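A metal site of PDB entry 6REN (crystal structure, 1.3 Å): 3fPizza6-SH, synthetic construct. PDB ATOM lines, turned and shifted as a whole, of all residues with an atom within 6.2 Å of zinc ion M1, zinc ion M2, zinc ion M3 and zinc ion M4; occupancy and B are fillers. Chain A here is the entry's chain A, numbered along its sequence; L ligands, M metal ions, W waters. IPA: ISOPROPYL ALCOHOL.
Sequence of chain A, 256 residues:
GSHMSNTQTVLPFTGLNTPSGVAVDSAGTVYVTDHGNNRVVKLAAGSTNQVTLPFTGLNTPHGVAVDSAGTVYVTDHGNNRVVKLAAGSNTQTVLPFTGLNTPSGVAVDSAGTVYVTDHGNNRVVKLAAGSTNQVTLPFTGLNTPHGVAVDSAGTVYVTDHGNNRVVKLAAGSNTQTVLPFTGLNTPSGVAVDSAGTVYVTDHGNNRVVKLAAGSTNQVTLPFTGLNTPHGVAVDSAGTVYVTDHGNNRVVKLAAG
Three residues have an atom within 4 Å of zinc ion M2: His 62, His 146 and His 230.
Of the 24 residues printed, 3 come within 4 Å of zinc ion M3.
The nearest printed residue that does not touch zinc ion M3 is Pro 229 (4.7 Å).
Zinc ion M2 is bound by NE2 of His 230 (2.0 Å), NE2 of His 146 (2.0 Å), NE2 of His 62 (2.0 Å) and water W1 (2.3 Å).
Zinc ion M4 is bound by O2 of IPA L3, NE2 of His 161, NE2 of His 119 and ND1 of His 146.
Zinc ion M4 has four donor atoms within binding distance.
Along chain A the residues within 4 Å of zinc ion M4 span positions 119 to 161.
The nearest printed residue that does not touch zinc ion M4 is Thr 144 (4.6 Å).
The backbone carbonyl oxygen (O) of His 62 sits close to the backbone NH (N) of Gly 21.
A ring nitrogen (ND1) of His 161 sits close to the side-chain hydroxyl (OG1) of Thr 144.
OG of Ser 104 sits at hydrogen-bond distance from O of His 146, at 2.8 Å.
A ring nitrogen (ND1) of His 77 lies close to the side-chain hydroxyl (OG1) of Thr 60 (3.2 Å).
The backbone carbonyl oxygen (O) of His 230 lies within hydrogen-bond range of the side-chain hydroxyl (OG) of Ser 188.
N of His 245 sits at hydrogen-bond distance from O of Thr 228 (3.1 Å).
N of Gly 189 is in hydrogen-bond range of O of His 230.
Zinc ion M3 is bound by O2 of IPA L2 (2.0 Å), NE2 of His 203 (2.0 Å), NE2 of His 245 (2.0 Å) and ND1 of His 230 (2.0 Å).
An oxygen (O2) of IPA L1 is bound to zinc ion M1.
NE2 of His 77 binds zinc ion M1.
Zinc ion M1 is bound by ND1 of His 62 (2.1 Å).
Zinc ion M1 is bound by a ring nitrogen (NE2) of His 35, 2.1 Å away.
Zinc ion M1 has four donor atoms within binding distance.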
ATOM      1  N   SER A  20       7.261  16.188   2.263  1.00  0.00           N
ATOM      2  CA  SER A  20       8.119  15.018   2.193  1.00  0.00           C
ATOM      3  C   SER A  20       8.838  14.770   3.508  1.00  0.00           C
ATOM      4  O   SER A  20       8.408  13.938   4.298  1.00  0.00           O
ATOM      5  CB  SER A  20       9.091  15.126   1.002  1.00  0.00           C
ATOM      6  OG  SER A  20       9.951  16.261   1.107  1.00  0.00           O
ATOM      7  N   GLY A  21       9.893  15.490   3.782  1.00  0.00           N
ATOM      8  CA  GLY A  21      10.584  15.292   5.033  1.00  0.00           C
ATOM      9  C   GLY A  21       9.842  15.890   6.225  1.00  0.00           C
ATOM     10  O   GLY A  21       9.146  16.910   6.116  1.00  0.00           O
ATOM     11  N   HIS A  35       8.019  20.062  -0.376  1.00  0.00           N
ATOM     12  CA  HIS A  35       8.908  19.701  -1.496  1.00  0.00           C
ATOM     13  C   HIS A  35       8.545  20.441  -2.770  1.00  0.00           C
ATOM     14  O   HIS A  35       9.440  20.942  -3.477  1.00  0.00           O
ATOM     15  CB  HIS A  35       8.764  18.188  -1.679  1.00  0.00           C
ATOM     16  CG  HIS A  35       9.743  17.468  -2.553  1.00  0.00           C
ATOM     17  ND1 HIS A  35       9.574  17.291  -3.918  1.00  0.00           N
ATOM     18  CD2 HIS A  35      10.793  16.676  -2.214  1.00  0.00           C
ATOM     19  CE1 HIS A  35      10.534  16.509  -4.383  1.00  0.00           C
ATOM     20  NE2 HIS A  35      11.292  16.104  -3.363  1.00  0.00           N
ATOM     21  N   THR A  60      13.378  21.396  -4.842  1.00  0.00           N
ATOM     22  CA  THR A  60      12.962  20.105  -4.307  1.00  0.00           C
ATOM     23  C   THR A  60      13.706  19.725  -3.019  1.00  0.00           C
ATOM     24  O   THR A  60      14.391  18.700  -2.949  1.00  0.00           O
ATOM     25  CB  THR A  60      12.969  18.953  -5.305  1.00  0.00           C
ATOM     26  OG1 THR A  60      14.231  18.815  -5.954  1.00  0.00           O
ATOM     27  CG2 THR A  60      11.903  19.224  -6.384  1.00  0.00           C
ATOM     28  N   PRO A  61      13.598  20.546  -1.974  1.00  0.00           N
ATOM     29  CA  PRO A  61      14.134  20.144  -0.658  1.00  0.00           C
ATOM     30  C   PRO A  61      13.407  18.913  -0.163  1.00  0.00           C
ATOM     31  O   PRO A  61      12.212  18.728  -0.387  1.00  0.00           O
ATOM     32  CB  PRO A  61      13.843  21.362   0.228  1.00  0.00           C
ATOM     33  CG  PRO A  61      12.604  21.962  -0.398  1.00  0.00           C
ATOM     34  CD  PRO A  61      12.746  21.758  -1.888  1.00  0.00           C
ATOM     35  N   HIS A  62      14.126  18.059   0.562  1.00  0.00           N
ATOM     36  CA  HIS A  62      13.584  16.727   0.833  1.00  0.00           C
ATOM     37  C   HIS A  62      13.778  16.372   2.313  1.00  0.00           C
ATOM     38  O   HIS A  62      12.896  16.581   3.126  1.00  0.00           O
ATOM     39  CB  HIS A  62      14.186  15.747  -0.166  1.00  0.00           C
ATOM     40  CG  HIS A  62      13.493  14.417  -0.194  1.00  0.00           C
ATOM     41  ND1 HIS A  62      12.896  13.917  -1.335  1.00  0.00           N
ATOM     42  CD2 HIS A  62      13.300  13.510   0.789  1.00  0.00           C
ATOM     43  CE1 HIS A  62      12.369  12.720  -1.049  1.00  0.00           C
ATOM     44  NE2 HIS A  62      12.594  12.471   0.238  1.00  0.00           N
ATOM     45  N   GLY A  63      14.934  15.914   2.735  1.00  0.00           N
ATOM     46  CA  GLY A  63      15.093  15.578   4.144  1.00  0.00           C
ATOM     47  C   GLY A  63      15.271  16.829   4.996  1.00  0.00           C
ATOM     48  O   GLY A  63      15.789  17.866   4.535  1.00  0.00           O
ATOM     49  N   HIS A  77      17.992  18.684  -2.851  1.00  0.00           N
ATOM     50  CA  HIS A  77      18.562  17.733  -3.822  1.00  0.00           C
ATOM     51  C   HIS A  77      18.642  18.259  -5.236  1.00  0.00           C
ATOM     52  O   HIS A  77      19.542  17.838  -5.957  1.00  0.00           O
ATOM     53  CB  HIS A  77      18.097  16.277  -3.762  1.00  0.00           C
ATOM     54  CG  HIS A  77      16.645  16.037  -4.025  1.00  0.00           C
ATOM     55  ND1 HIS A  77      16.045  16.237  -5.258  1.00  0.00           N
ATOM     56  CD2 HIS A  77      15.685  15.528  -3.226  1.00  0.00           C
ATOM     57  CE1 HIS A  77      14.781  15.861  -5.190  1.00  0.00           C
ATOM     58  NE2 HIS A  77      14.533  15.417  -3.972  1.00  0.00           N
ATOM     59  N   SER A 104      19.042  12.833  -0.272  1.00  0.00           N
ATOM     60  CA  SER A 104      17.637  12.737   0.133  1.00  0.00           C
ATOM     61  C   SER A 104      17.415  12.929   1.607  1.00  0.00           C
ATOM     62  O   SER A 104      16.403  13.514   1.983  1.00  0.00           O
ATOM     63  CB  SER A 104      17.026  11.418  -0.380  1.00  0.00           C
ATOM     64  OG  SER A 104      17.858  10.353   0.022  1.00  0.00           O
ATOM     65  N   HIS A 119      21.794   9.640  -2.079  1.00  0.00           N
ATOM     66  CA  HIS A 119      20.897   8.670  -2.712  1.00  0.00           C
ATOM     67  C   HIS A 119      21.437   8.203  -4.074  1.00  0.00           C
ATOM     68  O   HIS A 119      21.496   6.987  -4.363  1.00  0.00           O
ATOM     69  CB  HIS A 119      19.556   9.430  -2.829  1.00  0.00           C
ATOM     70  CG  HIS A 119      18.352   8.646  -3.263  1.00  0.00           C
ATOM     71  ND1 HIS A 119      18.056   8.368  -4.575  1.00  0.00           N
ATOM     72  CD2 HIS A 119      17.259   8.305  -2.539  1.00  0.00           C
ATOM     73  CE1 HIS A 119      16.847   7.822  -4.641  1.00  0.00           C
ATOM     74  NE2 HIS A 119      16.344   7.754  -3.416  1.00  0.00           N
ATOM     75  N   THR A 144      20.532   3.153  -3.704  1.00  0.00           N
ATOM     76  CA  THR A 144      19.663   4.300  -3.450  1.00  0.00           C
ATOM     77  C   THR A 144      19.201   4.391  -1.990  1.00  0.00           C
ATOM     78  O   THR A 144      17.998   4.337  -1.705  1.00  0.00           O
ATOM     79  CB  THR A 144      18.485   4.437  -4.421  1.00  0.00           C
ATOM     80  OG1 THR A 144      17.590   3.346  -4.248  1.00  0.00           O
ATOM     81  CG2 THR A 144      18.931   4.498  -5.856  1.00  0.00           C
ATOM     82  N   PRO A 145      20.135   4.525  -1.060  1.00  0.00           N
ATOM     83  CA  PRO A 145      19.752   4.781   0.340  1.00  0.00           C
ATOM     84  C   PRO A 145      19.025   6.132   0.439  1.00  0.00           C
ATOM     85  O   PRO A 145      19.443   7.123  -0.165  1.00  0.00           O
ATOM     86  CB  PRO A 145      21.103   4.813   1.069  1.00  0.00           C
ATOM     87  CG  PRO A 145      22.082   5.337  -0.013  1.00  0.00           C
ATOM     88  CD  PRO A 145      21.587   4.694  -1.303  1.00  0.00           C
ATOM     89  N   HIS A 146      17.942   6.151   1.207  1.00  0.00           N
ATOM     90  CA  HIS A 146      16.958   7.227   1.099  1.00  0.00           C
ATOM     91  C   HIS A 146      16.787   7.976   2.413  1.00  0.00           C
ATOM     92  O   HIS A 146      17.166   9.162   2.493  1.00  0.00           O
ATOM     93  CB  HIS A 146      15.647   6.632   0.557  1.00  0.00           C
ATOM     94  CG  HIS A 146      14.564   7.653   0.317  1.00  0.00           C
ATOM     95  ND1 HIS A 146      14.107   7.999  -0.935  1.00  0.00           N
ATOM     96  CD2 HIS A 146      13.890   8.441   1.206  1.00  0.00           C
ATOM     97  CE1 HIS A 146      13.188   8.935  -0.809  1.00  0.00           C
ATOM     98  NE2 HIS A 146      13.027   9.236   0.471  1.00  0.00           N
ATOM     99  N   GLY A 147      16.221   7.343   3.437  1.00  0.00           N
ATOM    100  CA  GLY A 147      16.015   7.955   4.736  1.00  0.00           C
ATOM    101  C   GLY A 147      17.175   7.608   5.650  1.00  0.00           C
ATOM    102  O   GLY A 147      17.787   6.544   5.514  1.00  0.00           O
ATOM    103  N   HIS A 161      16.457   1.444  -0.064  1.00  0.00           N
ATOM    104  CA  HIS A 161      15.273   0.930  -0.757  1.00  0.00           C
ATOM    105  C   HIS A 161      15.586   0.257  -2.083  1.00  0.00           C
ATOM    106  O   HIS A 161      14.753  -0.525  -2.536  1.00  0.00           O
ATOM    107  CB  HIS A 161      14.088   1.927  -0.812  1.00  0.00           C
ATOM    108  CG  HIS A 161      14.281   3.111  -1.743  1.00  0.00           C
ATOM    109  ND1 HIS A 161      14.455   3.015  -3.115  1.00  0.00           N
ATOM    110  CD2 HIS A 161      14.208   4.435  -1.475  1.00  0.00           C
ATOM    111  CE1 HIS A 161      14.547   4.239  -3.635  1.00  0.00           C
ATOM    112  NE2 HIS A 161      14.398   5.129  -2.657  1.00  0.00           N
ATOM    113  N   PRO A 187      10.883   1.173   1.231  1.00  0.00           N
ATOM    114  CA  PRO A 187      10.767   2.094   2.376  1.00  0.00           C
ATOM    115  C   PRO A 187      11.384   3.466   2.109  1.00  0.00           C
ATOM    116  O   PRO A 187      12.393   3.586   1.400  1.00  0.00           O
ATOM    117  CB  PRO A 187      11.515   1.363   3.489  1.00  0.00           C
ATOM    118  CG  PRO A 187      12.515   0.510   2.770  1.00  0.00           C
ATOM    119  CD  PRO A 187      11.799   0.046   1.517  1.00  0.00           C
ATOM    120  N   SER A 188      10.763   4.495   2.712  1.00  0.00           N
ATOM    121  CA  SER A 188      11.231   5.891   2.557  1.00  0.00           C
ATOM    122  C   SER A 188      11.698   6.447   3.907  1.00  0.00           C
ATOM    123  O   SER A 188      12.879   6.348   4.241  1.00  0.00           O
ATOM    124  CB  SER A 188      10.150   6.758   1.880  1.00  0.00           C
ATOM    125  OG  SER A 188       8.871   6.600   2.529  1.00  0.00           O
ATOM    126  N   GLY A 189      10.846   7.082   4.696  1.00  0.00           N
ATOM    127  CA  GLY A 189      11.308   7.658   5.953  1.00  0.00           C
ATOM    128  C   GLY A 189      11.658   6.598   6.979  1.00  0.00           C
ATOM    129  O   GLY A 189      11.081   5.502   7.025  1.00  0.00           O
ATOM    130  N   HIS A 203       6.556   2.769   2.003  1.00  0.00           N
ATOM    131  CA  HIS A 203       5.905   3.658   1.041  1.00  0.00           C
ATOM    132  C   HIS A 203       5.051   2.900   0.043  1.00  0.00           C
ATOM    133  O   HIS A 203       3.952   3.332  -0.297  1.00  0.00           O
ATOM    134  CB  HIS A 203       7.005   4.467   0.329  1.00  0.00           C
ATOM    135  CG  HIS A 203       6.536   5.694  -0.400  1.00  0.00           C
ATOM    136  ND1 HIS A 203       5.722   5.677  -1.525  1.00  0.00           N
ATOM    137  CD2 HIS A 203       6.836   6.997  -0.179  1.00  0.00           C
ATOM    138  CE1 HIS A 203       5.543   6.928  -1.952  1.00  0.00           C
ATOM    139  NE2 HIS A 203       6.241   7.747  -1.178  1.00  0.00           N
ATOM    140  N   THR A 228      -0.794   8.616   0.708  1.00  0.00           N
ATOM    141  CA  THR A 228       0.577   8.301   0.276  1.00  0.00           C
ATOM    142  C   THR A 228       1.561   8.827   1.325  1.00  0.00           C
ATOM    143  O   THR A 228       2.199   9.876   1.141  1.00  0.00           O
ATOM    144  CB  THR A 228       0.857   8.850  -1.135  1.00  0.00           C
ATOM    145  OG1 THR A 228      -0.193   8.424  -2.022  1.00  0.00           O
ATOM    146  CG2 THR A 228       2.175   8.344  -1.697  1.00  0.00           C
ATOM    147  N   PRO A 229       1.699   8.146   2.447  1.00  0.00           N
ATOM    148  CA  PRO A 229       2.662   8.586   3.476  1.00  0.00           C
ATOM    149  C   PRO A 229       4.096   8.484   2.970  1.00  0.00           C
ATOM    150  O   PRO A 229       4.433   7.658   2.102  1.00  0.00           O
ATOM    151  CB  PRO A 229       2.403   7.608   4.628  1.00  0.00           C
ATOM    152  CG  PRO A 229       1.859   6.353   3.956  1.00  0.00           C
ATOM    153  CD  PRO A 229       0.979   6.917   2.852  1.00  0.00           C
ATOM    154  N   HIS A 230       4.974   9.342   3.525  1.00  0.00           N
ATOM    155  CA  HIS A 230       6.335   9.434   3.021  1.00  0.00           C
ATOM    156  C   HIS A 230       7.358   9.556   4.141  1.00  0.00           C
ATOM    157  O   HIS A 230       8.203   8.664   4.333  1.00  0.00           O
ATOM    158  CB  HIS A 230       6.470  10.559   1.976  1.00  0.00           C
ATOM    159  CG  HIS A 230       7.817  10.564   1.331  1.00  0.00           C
ATOM    160  ND1 HIS A 230       8.059  10.170   0.039  1.00  0.00           N
ATOM    161  CD2 HIS A 230       9.028  10.883   1.863  1.00  0.00           C
ATOM    162  CE1 HIS A 230       9.376  10.203  -0.187  1.00  0.00           C
ATOM    163  NE2 HIS A 230      10.000  10.630   0.911  1.00  0.00           N
ATOM    164  N   GLY A 231       7.345  10.669   4.861  1.00  0.00           N
ATOM    165  CA  GLY A 231       8.304  10.891   5.932  1.00  0.00           C
ATOM    166  C   GLY A 231       7.720  10.521   7.281  1.00  0.00           C
ATOM    167  O   GLY A 231       6.485  10.546   7.478  1.00  0.00           O
ATOM    168  N   HIS A 245       1.860  12.968   1.092  1.00  0.00           N
ATOM    169  CA  HIS A 245       1.794  13.779  -0.126  1.00  0.00           C
ATOM    170  C   HIS A 245       0.704  13.331  -1.080  1.00  0.00           C
ATOM    171  O   HIS A 245       0.545  13.944  -2.145  1.00  0.00           O
ATOM    172  CB  HIS A 245       3.158  13.963  -0.821  1.00  0.00           C
ATOM    173  CG  HIS A 245       3.853  12.696  -1.259  1.00  0.00           C
ATOM    174  ND1 HIS A 245       3.403  11.912  -2.294  1.00  0.00           N
ATOM    175  CD2 HIS A 245       4.993  12.118  -0.814  1.00  0.00           C
ATOM    176  CE1 HIS A 245       4.221  10.890  -2.450  1.00  0.00           C
ATOM    177  NE2 HIS A 245       5.208  10.985  -1.567  1.00  0.00           N
HETATM  178  C1  IPA L   1      11.406  12.165  -6.450  1.00  0.00           C
HETATM  179  C2  IPA L   1      11.580  13.441  -5.640  1.00  0.00           C
HETATM  180  C3  IPA L   1      12.220  14.525  -6.491  1.00  0.00           C
HETATM  181  O2  IPA L   1      12.202  13.235  -4.386  1.00  0.00           O
HETATM  182  C1  IPA L   2       6.166   9.137  -4.175  1.00  0.00           C
HETATM  183  C2  IPA L   2       7.639   9.279  -4.214  1.00  0.00           C
HETATM  184  C3  IPA L   2       8.306   9.736  -5.493  1.00  0.00           C
HETATM  185  O2  IPA L   2       8.006   9.776  -3.017  1.00  0.00           O
HETATM  186  C1  IPA L   3      14.088   6.663  -5.563  1.00  0.00           C
HETATM  187  C2  IPA L   3      13.113   7.640  -5.159  1.00  0.00           C
HETATM  188  C3  IPA L   3      12.026   8.029  -6.139  1.00  0.00           C
HETATM  189  O2  IPA L   3      13.040   7.972  -3.874  1.00  0.00           O
HETATM  190 ZN    ZN M   1      12.788  14.707  -3.224  1.00  0.00          ZN
HETATM  191 ZN    ZN M   2      11.956  10.790   1.191  1.00  0.00          ZN
HETATM  192 ZN    ZN M   3       6.764   9.672  -1.469  1.00  0.00          ZN
HETATM  193 ZN    ZN M   4      14.493   7.153  -2.768  1.00  0.00          ZN
HETATM  194  O   HOH W   1      12.071  10.775   3.533  1.00  0.00           O
